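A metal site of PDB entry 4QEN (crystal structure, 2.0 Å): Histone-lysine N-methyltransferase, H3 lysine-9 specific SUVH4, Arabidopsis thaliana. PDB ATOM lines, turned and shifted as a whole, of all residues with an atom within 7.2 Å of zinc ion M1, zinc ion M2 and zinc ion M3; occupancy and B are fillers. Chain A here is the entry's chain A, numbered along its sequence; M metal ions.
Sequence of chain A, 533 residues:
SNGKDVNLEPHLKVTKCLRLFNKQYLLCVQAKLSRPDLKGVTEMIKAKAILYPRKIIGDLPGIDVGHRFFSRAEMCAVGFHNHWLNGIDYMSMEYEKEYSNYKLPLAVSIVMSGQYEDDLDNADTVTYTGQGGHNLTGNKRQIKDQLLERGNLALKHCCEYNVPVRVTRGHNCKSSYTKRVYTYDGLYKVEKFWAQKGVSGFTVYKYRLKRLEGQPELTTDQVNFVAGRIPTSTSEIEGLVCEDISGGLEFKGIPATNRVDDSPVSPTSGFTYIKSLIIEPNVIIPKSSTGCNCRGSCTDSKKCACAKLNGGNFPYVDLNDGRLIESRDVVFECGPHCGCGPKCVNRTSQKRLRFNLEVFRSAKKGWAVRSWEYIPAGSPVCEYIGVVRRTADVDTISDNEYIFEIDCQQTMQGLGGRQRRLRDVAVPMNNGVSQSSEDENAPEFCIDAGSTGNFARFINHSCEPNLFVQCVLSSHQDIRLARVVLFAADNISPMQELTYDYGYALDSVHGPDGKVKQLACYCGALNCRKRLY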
ATOM      1  N   THR A 290     -18.903 -13.061  22.005  1.00  0.00           N
ATOM      2  CA  THR A 290     -20.137 -12.616  22.624  1.00  0.00           C
ATOM      3  C   THR A 290     -21.276 -12.450  21.608  1.00  0.00           C
ATOM      4  O   THR A 290     -22.410 -12.859  21.853  1.00  0.00           O
ATOM      5  CB  THR A 290     -19.921 -11.301  23.394  1.00  0.00           C
ATOM      6  OG1 THR A 290     -18.933 -11.504  24.408  1.00  0.00           O
ATOM      7  CG2 THR A 290     -21.210 -10.829  24.024  1.00  0.00           C
ATOM      8  N   GLY A 291     -20.977 -11.840  20.461  1.00  0.00           N
ATOM      9  CA  GLY A 291     -21.990 -11.673  19.430  1.00  0.00           C
ATOM     10  C   GLY A 291     -22.942 -10.494  19.631  1.00  0.00           C
ATOM     11  O   GLY A 291     -22.833  -9.729  20.584  1.00  0.00           O
ATOM     12  N   CYS A 292     -23.903 -10.371  18.712  1.00  0.00           N
ATOM     13  CA  CYS A 292     -24.804  -9.221  18.698  1.00  0.00           C
ATOM     14  C   CYS A 292     -26.201  -9.671  19.106  1.00  0.00           C
ATOM     15  O   CYS A 292     -26.470 -10.878  19.175  1.00  0.00           O
ATOM     16  CB  CYS A 292     -24.853  -8.616  17.283  1.00  0.00           C
ATOM     17  SG  CYS A 292     -25.544  -9.727  16.020  1.00  0.00           S
ATOM     18  N   ASN A 293     -27.091  -8.725  19.352  1.00  0.00           N
ATOM     19  CA  ASN A 293     -28.423  -9.071  19.841  1.00  0.00           C
ATOM     20  C   ASN A 293     -29.503  -8.826  18.805  1.00  0.00           C
ATOM     21  O   ASN A 293     -30.693  -8.805  19.131  1.00  0.00           O
ATOM     22  CB  ASN A 293     -28.745  -8.348  21.163  1.00  0.00           C
ATOM     23  CG  ASN A 293     -28.724  -6.831  21.027  1.00  0.00           C
ATOM     24  OD1 ASN A 293     -28.790  -6.283  19.930  1.00  0.00           O
ATOM     25  ND2 ASN A 293     -28.635  -6.142  22.166  1.00  0.00           N
ATOM     26  N   CYS A 294     -29.072  -8.608  17.563  1.00  0.00           N
ATOM     27  CA  CYS A 294     -29.996  -8.368  16.475  1.00  0.00           C
ATOM     28  C   CYS A 294     -30.878  -9.591  16.286  1.00  0.00           C
ATOM     29  O   CYS A 294     -30.514 -10.692  16.692  1.00  0.00           O
ATOM     30  CB  CYS A 294     -29.241  -8.067  15.171  1.00  0.00           C
ATOM     31  SG  CYS A 294     -28.016  -6.733  15.314  1.00  0.00           S
ATOM     32  N   ARG A 295     -32.032  -9.399  15.671  1.00  0.00           N
ATOM     33  CA  ARG A 295     -32.959 -10.495  15.484  1.00  0.00           C
ATOM     34  C   ARG A 295     -33.215 -10.775  14.010  1.00  0.00           C
ATOM     35  O   ARG A 295     -33.559  -9.878  13.250  1.00  0.00           O
ATOM     36  CB  ARG A 295     -34.271 -10.209  16.207  1.00  0.00           C
ATOM     37  CG  ARG A 295     -35.045 -11.443  16.568  1.00  0.00           C
ATOM     38  CD  ARG A 295     -36.002 -11.176  17.699  1.00  0.00           C
ATOM     39  NE  ARG A 295     -37.142 -12.073  17.650  1.00  0.00           N
ATOM     40  CZ  ARG A 295     -37.121 -13.334  18.058  1.00  0.00           C
ATOM     41  NH1 ARG A 295     -38.207 -14.080  17.970  1.00  0.00           N
ATOM     42  NH2 ARG A 295     -36.005 -13.842  18.562  1.00  0.00           N
ATOM     43  N   GLY A 296     -33.035 -12.030  13.612  1.00  0.00           N
ATOM     44  CA  GLY A 296     -33.298 -12.426  12.239  1.00  0.00           C
ATOM     45  C   GLY A 296     -32.127 -12.179  11.320  1.00  0.00           C
ATOM     46  O   GLY A 296     -31.406 -13.118  10.986  1.00  0.00           O
ATOM     47  N   SER A 297     -31.957 -10.936  10.895  1.00  0.00           N
ATOM     48  CA  SER A 297     -30.825 -10.543  10.049  1.00  0.00           C
ATOM     49  C   SER A 297     -30.250  -9.239  10.554  1.00  0.00           C
ATOM     50  O   SER A 297     -30.995  -8.359  10.983  1.00  0.00           O
ATOM     51  CB  SER A 297     -31.264 -10.366   8.599  1.00  0.00           C
ATOM     52  OG  SER A 297     -31.444 -11.612   7.946  1.00  0.00           O
ATOM     53  N   CYS A 298     -28.941  -9.080  10.483  1.00  0.00           N
ATOM     54  CA  CYS A 298     -28.340  -7.824  10.931  1.00  0.00           C
ATOM     55  C   CYS A 298     -28.323  -6.773   9.818  1.00  0.00           C
ATOM     56  O   CYS A 298     -27.726  -6.989   8.769  1.00  0.00           O
ATOM     57  CB  CYS A 298     -26.939  -8.068  11.477  1.00  0.00           C
ATOM     58  SG  CYS A 298     -26.997  -9.238  12.809  1.00  0.00           S
ATOM     59  N   THR A 299     -29.015  -5.655  10.059  1.00  0.00           N
ATOM     60  CA  THR A 299     -29.139  -4.607   9.035  1.00  0.00           C
ATOM     61  C   THR A 299     -28.844  -3.201   9.556  1.00  0.00           C
ATOM     62  O   THR A 299     -28.505  -2.302   8.785  1.00  0.00           O
ATOM     63  CB  THR A 299     -30.536  -4.594   8.382  1.00  0.00           C
ATOM     64  OG1 THR A 299     -31.529  -4.658   9.412  1.00  0.00           O
ATOM     65  CG2 THR A 299     -30.699  -5.792   7.452  1.00  0.00           C
ATOM     66  N   ASP A 300     -28.980  -3.006  10.861  1.00  0.00           N
ATOM     67  CA  ASP A 300     -28.695  -1.715  11.464  1.00  0.00           C
ATOM     68  C   ASP A 300     -27.294  -1.727  12.065  1.00  0.00           C
ATOM     69  O   ASP A 300     -27.046  -2.349  13.094  1.00  0.00           O
ATOM     70  CB  ASP A 300     -29.747  -1.384  12.524  1.00  0.00           C
ATOM     71  CG  ASP A 300     -29.624   0.034  13.049  1.00  0.00           C
ATOM     72  OD1 ASP A 300     -28.497   0.472  13.356  1.00  0.00           O
ATOM     73  OD2 ASP A 300     -30.668   0.727  13.146  1.00  0.00           O
ATOM     74  N   LYS A 303     -26.864  -0.600  15.857  1.00  0.00           N
ATOM     75  CA  LYS A 303     -27.293  -1.471  16.943  1.00  0.00           C
ATOM     76  C   LYS A 303     -26.478  -2.765  17.021  1.00  0.00           C
ATOM     77  O   LYS A 303     -26.496  -3.440  18.050  1.00  0.00           O
ATOM     78  CB  LYS A 303     -28.785  -1.811  16.801  1.00  0.00           C
ATOM     79  CG  LYS A 303     -29.697  -0.596  16.700  1.00  0.00           C
ATOM     80  CD  LYS A 303     -31.136  -0.975  17.046  1.00  0.00           C
ATOM     81  CE  LYS A 303     -32.146  -0.258  16.148  1.00  0.00           C
ATOM     82  NZ  LYS A 303     -32.096  -0.791  14.741  1.00  0.00           N
ATOM     83  N   CYS A 304     -25.791  -3.100  15.941  1.00  0.00           N
ATOM     84  CA  CYS A 304     -25.106  -4.390  15.800  1.00  0.00           C
ATOM     85  C   CYS A 304     -23.654  -4.376  16.259  1.00  0.00           C
ATOM     86  O   CYS A 304     -22.806  -3.744  15.636  1.00  0.00           O
ATOM     87  CB  CYS A 304     -25.167  -4.852  14.345  1.00  0.00           C
ATOM     88  SG  CYS A 304     -24.316  -6.441  14.032  1.00  0.00           S
ATOM     89  N   ALA A 305     -23.365  -5.098  17.339  1.00  0.00           N
ATOM     90  CA  ALA A 305     -21.999  -5.200  17.864  1.00  0.00           C
ATOM     91  C   ALA A 305     -21.002  -5.766  16.840  1.00  0.00           C
ATOM     92  O   ALA A 305     -19.796  -5.463  16.875  1.00  0.00           O
ATOM     93  CB  ALA A 305     -21.994  -6.050  19.140  1.00  0.00           C
ATOM     94  N   CYS A 306     -21.507  -6.579  15.924  1.00  0.00           N
ATOM     95  CA  CYS A 306     -20.661  -7.218  14.929  1.00  0.00           C
ATOM     96  C   CYS A 306     -20.283  -6.232  13.815  1.00  0.00           C
ATOM     97  O   CYS A 306     -19.176  -6.292  13.280  1.00  0.00           O
ATOM     98  CB  CYS A 306     -21.332  -8.479  14.382  1.00  0.00           C
ATOM     99  SG  CYS A 306     -21.680  -9.757  15.657  1.00  0.00           S
ATOM    100  N   ALA A 307     -21.183  -5.316  13.491  1.00  0.00           N
ATOM    101  CA  ALA A 307     -20.845  -4.216  12.591  1.00  0.00           C
ATOM    102  C   ALA A 307     -19.817  -3.314  13.274  1.00  0.00           C
ATOM    103  O   ALA A 307     -18.901  -2.808  12.625  1.00  0.00           O
ATOM    104  CB  ALA A 307     -22.100  -3.416  12.212  1.00  0.00           C
ATOM    105  N   PHE A 314     -21.024  -2.834   7.752  1.00  0.00           N
ATOM    106  CA  PHE A 314     -20.944  -4.239   7.381  1.00  0.00           C
ATOM    107  C   PHE A 314     -19.929  -4.406   6.260  1.00  0.00           C
ATOM    108  O   PHE A 314     -19.860  -3.578   5.357  1.00  0.00           O
ATOM    109  CB  PHE A 314     -22.326  -4.755   6.979  1.00  0.00           C
ATOM    110  CG  PHE A 314     -23.294  -4.821   8.136  1.00  0.00           C
ATOM    111  CD1 PHE A 314     -23.228  -5.860   9.050  1.00  0.00           C
ATOM    112  CD2 PHE A 314     -24.249  -3.839   8.314  1.00  0.00           C
ATOM    113  CE1 PHE A 314     -24.118  -5.917  10.131  1.00  0.00           C
ATOM    114  CE2 PHE A 314     -25.142  -3.896   9.375  1.00  0.00           C
ATOM    115  CZ  PHE A 314     -25.062  -4.934  10.286  1.00  0.00           C
ATOM    116  N   PHE A 332     -15.124  -9.543  10.632  1.00  0.00           N
ATOM    117  CA  PHE A 332     -15.825 -10.101  11.788  1.00  0.00           C
ATOM    118  C   PHE A 332     -17.252 -10.485  11.428  1.00  0.00           C
ATOM    119  O   PHE A 332     -18.100  -9.613  11.216  1.00  0.00           O
ATOM    120  CB  PHE A 332     -15.838  -9.102  12.943  1.00  0.00           C
ATOM    121  CG  PHE A 332     -14.474  -8.795  13.496  1.00  0.00           C
ATOM    122  CD1 PHE A 332     -13.954  -9.534  14.541  1.00  0.00           C
ATOM    123  CD2 PHE A 332     -13.721  -7.748  12.973  1.00  0.00           C
ATOM    124  CE1 PHE A 332     -12.698  -9.241  15.054  1.00  0.00           C
ATOM    125  CE2 PHE A 332     -12.474  -7.448  13.478  1.00  0.00           C
ATOM    126  CZ  PHE A 332     -11.961  -8.195  14.523  1.00  0.00           C
ATOM    127  N   GLU A 333     -17.514 -11.780  11.341  1.00  0.00           N
ATOM    128  CA  GLU A 333     -18.846 -12.291  11.011  1.00  0.00           C
ATOM    129  C   GLU A 333     -19.655 -12.591  12.265  1.00  0.00           C
ATOM    130  O   GLU A 333     -19.082 -12.807  13.330  1.00  0.00           O
ATOM    131  CB  GLU A 333     -18.747 -13.557  10.160  1.00  0.00           C
ATOM    132  CG  GLU A 333     -18.527 -13.280   8.665  1.00  0.00           C
ATOM    133  CD  GLU A 333     -18.445 -14.554   7.838  1.00  0.00           C
ATOM    134  OE1 GLU A 333     -18.548 -15.672   8.395  1.00  0.00           O
ATOM    135  OE2 GLU A 333     -18.269 -14.425   6.613  1.00  0.00           O
ATOM    136  N   CYS A 334     -20.979 -12.617  12.127  1.00  0.00           N
ATOM    137  CA  CYS A 334     -21.855 -13.077  13.207  1.00  0.00           C
ATOM    138  C   CYS A 334     -21.553 -14.558  13.484  1.00  0.00           C
ATOM    139  O   CYS A 334     -21.030 -15.260  12.602  1.00  0.00           O
ATOM    140  CB  CYS A 334     -23.320 -12.853  12.847  1.00  0.00           C
ATOM    141  SG  CYS A 334     -23.746 -11.101  12.733  1.00  0.00           S
ATOM    142  N   GLY A 335     -21.855 -15.014  14.696  1.00  0.00           N
ATOM    143  CA  GLY A 335     -21.461 -16.349  15.121  1.00  0.00           C
ATOM    144  C   GLY A 335     -22.497 -17.039  15.993  1.00  0.00           C
ATOM    145  O   GLY A 335     -23.659 -16.636  16.016  1.00  0.00           O
ATOM    146  N   HIS A 337     -23.421 -17.162  18.986  1.00  0.00           N
ATOM    147  CA  HIS A 337     -24.209 -16.488  20.021  1.00  0.00           C
ATOM    148  C   HIS A 337     -24.961 -15.268  19.521  1.00  0.00           C
ATOM    149  O   HIS A 337     -25.634 -14.594  20.300  1.00  0.00           O
ATOM    150  CB  HIS A 337     -23.331 -16.123  21.222  1.00  0.00           C
ATOM    151  CG  HIS A 337     -22.832 -17.309  21.976  1.00  0.00           C
ATOM    152  ND1 HIS A 337     -23.670 -18.203  22.591  1.00  0.00           N
ATOM    153  CD2 HIS A 337     -21.569 -17.752  22.208  1.00  0.00           C
ATOM    154  CE1 HIS A 337     -22.963 -19.156  23.176  1.00  0.00           C
ATOM    155  NE2 HIS A 337     -21.676 -18.902  22.959  1.00  0.00           N
ATOM    156  N   CYS A 338     -24.852 -14.975  18.232  1.00  0.00           N
ATOM    157  CA  CYS A 338     -25.609 -13.840  17.701  1.00  0.00           C
ATOM    158  C   CYS A 338     -27.096 -14.182  17.660  1.00  0.00           C
ATOM    159  O   CYS A 338     -27.464 -15.344  17.525  1.00  0.00           O
ATOM    160  CB  CYS A 338     -25.093 -13.449  16.323  1.00  0.00           C
ATOM    161  SG  CYS A 338     -23.403 -12.822  16.391  1.00  0.00           S
ATOM    162  N   GLY A 339     -27.940 -13.177  17.775  1.00  0.00           N
ATOM    163  CA  GLY A 339     -29.380 -13.398  17.728  1.00  0.00           C
ATOM    164  C   GLY A 339     -29.912 -13.612  16.319  1.00  0.00           C
ATOM    165  O   GLY A 339     -31.086 -13.968  16.145  1.00  0.00           O
ATOM    166  N   CYS A 340     -29.075 -13.409  15.313  1.00  0.00           N
ATOM    167  CA  CYS A 340     -29.511 -13.517  13.928  1.00  0.00           C
ATOM    168  C   CYS A 340     -29.414 -14.947  13.421  1.00  0.00           C
ATOM    169  O   CYS A 340     -28.637 -15.742  13.935  1.00  0.00           O
ATOM    170  CB  CYS A 340     -28.642 -12.630  13.032  1.00  0.00           C
ATOM    171  SG  CYS A 340     -26.904 -13.106  13.108  1.00  0.00           S
ATOM    172  N   GLY A 341     -30.208 -15.251  12.398  1.00  0.00           N
ATOM    173  CA  GLY A 341     -30.221 -16.567  11.782  1.00  0.00           C
ATOM    174  C   GLY A 341     -29.288 -16.641  10.578  1.00  0.00           C
ATOM    175  O   GLY A 341     -28.614 -15.656  10.242  1.00  0.00           O
ATOM    176  N   LYS A 343     -29.500 -16.515   7.452  1.00  0.00           N
ATOM    177  CA  LYS A 343     -29.665 -15.648   6.279  1.00  0.00           C
ATOM    178  C   LYS A 343     -28.925 -14.327   6.416  1.00  0.00           C
ATOM    179  O   LYS A 343     -28.749 -13.616   5.428  1.00  0.00           O
ATOM    180  CB  LYS A 343     -31.150 -15.376   6.006  1.00  0.00           C
ATOM    181  CG  LYS A 343     -31.900 -16.545   5.395  1.00  0.00           C
ATOM    182  CD  LYS A 343     -33.297 -16.120   4.955  1.00  0.00           C
ATOM    183  CE  LYS A 343     -34.088 -17.298   4.393  1.00  0.00           C
ATOM    184  NZ  LYS A 343     -35.489 -16.918   4.075  1.00  0.00           N
ATOM    185  N   CYS A 344     -28.483 -14.003   7.631  1.00  0.00           N
ATOM    186  CA  CYS A 344     -27.762 -12.755   7.882  1.00  0.00           C
ATOM    187  C   CYS A 344     -26.628 -12.500   6.889  1.00  0.00           C
ATOM    188  O   CYS A 344     -25.820 -13.389   6.600  1.00  0.00           O
ATOM    189  CB  CYS A 344     -27.196 -12.725   9.300  1.00  0.00           C
ATOM    190  SG  CYS A 344     -26.346 -11.195   9.644  1.00  0.00           S
ATOM    191  N   VAL A 345     -26.571 -11.292   6.363  1.00  0.00           N
ATOM    192  CA  VAL A 345     -25.558 -10.980   5.345  1.00  0.00           C
ATOM    193  C   VAL A 345     -24.158 -10.971   5.977  1.00  0.00           C
ATOM    194  O   VAL A 345     -23.157 -11.298   5.325  1.00  0.00           O
ATOM    195  CB  VAL A 345     -25.864  -9.652   4.627  1.00  0.00           C
ATOM    196  CG1 VAL A 345     -24.809  -9.332   3.570  1.00  0.00           C
ATOM    197  CG2 VAL A 345     -27.248  -9.752   3.959  1.00  0.00           C
ATOM    198  N   ASN A 346     -24.097 -10.675   7.266  1.00  0.00           N
ATOM    199  CA  ASN A 346     -22.838 -10.754   7.985  1.00  0.00           C
ATOM    200  C   ASN A 346     -22.479 -12.202   8.373  1.00  0.00           C
ATOM    201  O   ASN A 346     -21.641 -12.424   9.244  1.00  0.00           O
ATOM    202  CB  ASN A 346     -22.846  -9.820   9.198  1.00  0.00           C
ATOM    203  CG  ASN A 346     -21.451  -9.374   9.586  1.00  0.00           C
ATOM    204  OD1 ASN A 346     -20.637  -9.083   8.728  1.00  0.00           O
ATOM    205  ND2 ASN A 346     -21.165  -9.345  10.896  1.00  0.00           N
ATOM    206  N   ARG A 347     -23.112 -13.178   7.744  1.00  0.00           N
ATOM    207  CA  ARG A 347     -22.642 -14.553   7.786  1.00  0.00           C
ATOM    208  C   ARG A 347     -22.349 -15.040   6.373  1.00  0.00           C
ATOM    209  O   ARG A 347     -22.444 -16.237   6.081  1.00  0.00           O
ATOM    210  CB  ARG A 347     -23.679 -15.492   8.409  1.00  0.00           C
ATOM    211  CG  ARG A 347     -24.042 -15.183   9.852  1.00  0.00           C
ATOM    212  CD  ARG A 347     -25.181 -16.084  10.292  1.00  0.00           C
ATOM    213  NE  ARG A 347     -25.639 -15.823  11.651  1.00  0.00           N
ATOM    214  CZ  ARG A 347     -25.110 -16.415  12.718  1.00  0.00           C
ATOM    215  NH1 ARG A 347     -24.112 -17.269  12.555  1.00  0.00           N
ATOM    216  NH2 ARG A 347     -25.588 -16.158  13.938  1.00  0.00           N
HETATM  217 ZN    ZN M   1     -26.110  -7.951  14.496  1.00  0.00          ZN
HETATM  218 ZN    ZN M   2     -23.635 -10.737  15.124  1.00  0.00          ZN
HETATM  219 ZN    ZN M   3     -25.973 -11.295  12.015  1.00  0.00          ZN
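N of Cys 306 lies close to SG of Cys 304.
O of Cys 294 lies within hydrogen-bond range of N of Cys 340.
NH2 of Arg 347 is in hydrogen-bond range of O of Cys 340 (3.1 Å).
The backbone NH (N) of Gly 339 is in hydrogen-bond range of the backbone carbonyl oxygen (O) of Cys 292, 3.1 Å away.
The backbone NH (N) of Cys 334 sits at hydrogen-bond distance from the backbone carbonyl oxygen (O) of Asn 346.
The side-chain sulfur (SG) of Cys 304 lies close to the backbone NH (N) of Ala 307 (3.4 Å).
SG of Cys 344 lies close to N of Asn 346.
The side-chain sulfur (SG) of Cys 338 lies close to the backbone NH (N) of Gly 335 (3.2 Å).
Within 4 Å of zinc ion M1: Cys 292, Cys 294, Cys 298 and Cys 304.
Within 4 Å of zinc ion M2: Cys 292, Cys 306, Cys 334 and Cys 338.
Of the 31 residues printed, 4 come within 4 Å of zinc ion M3.
The nearest printed residue that does not touch zinc ion M3 is Cys 292 (4.3 Å).
The side-chain sulfur (SG) of Cys 298 binds zinc ion M1 (2.3 Å).
Zinc ion M1 is bound by SG of Cys 304, at 2.4 Å.
The side-chain sulfur (SG) of Cys 294 is bound to zinc ion M1.
Zinc ion M1 is bound by SG of Cys 292 (2.4 Å).
Zinc ion M2 is bound by SG of Cys 306 (2.3 Å), SG of Cys 292 (2.3 Å), SG of Cys 334 (2.4 Å) and SG of Cys 338 (2.5 Å).
Zinc ion M3 is bound by the side-chain sulfur (SG) of Cys 340 (2.3 Å), the side-chain sulfur (SG) of Cys 334 (2.3 Å), the side-chain sulfur (SG) of Cys 344 (2.4 Å) and the side-chain sulfur (SG) of Cys 298 (2.4 Å).
Zinc ion M3 has four donor atoms within binding distance.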
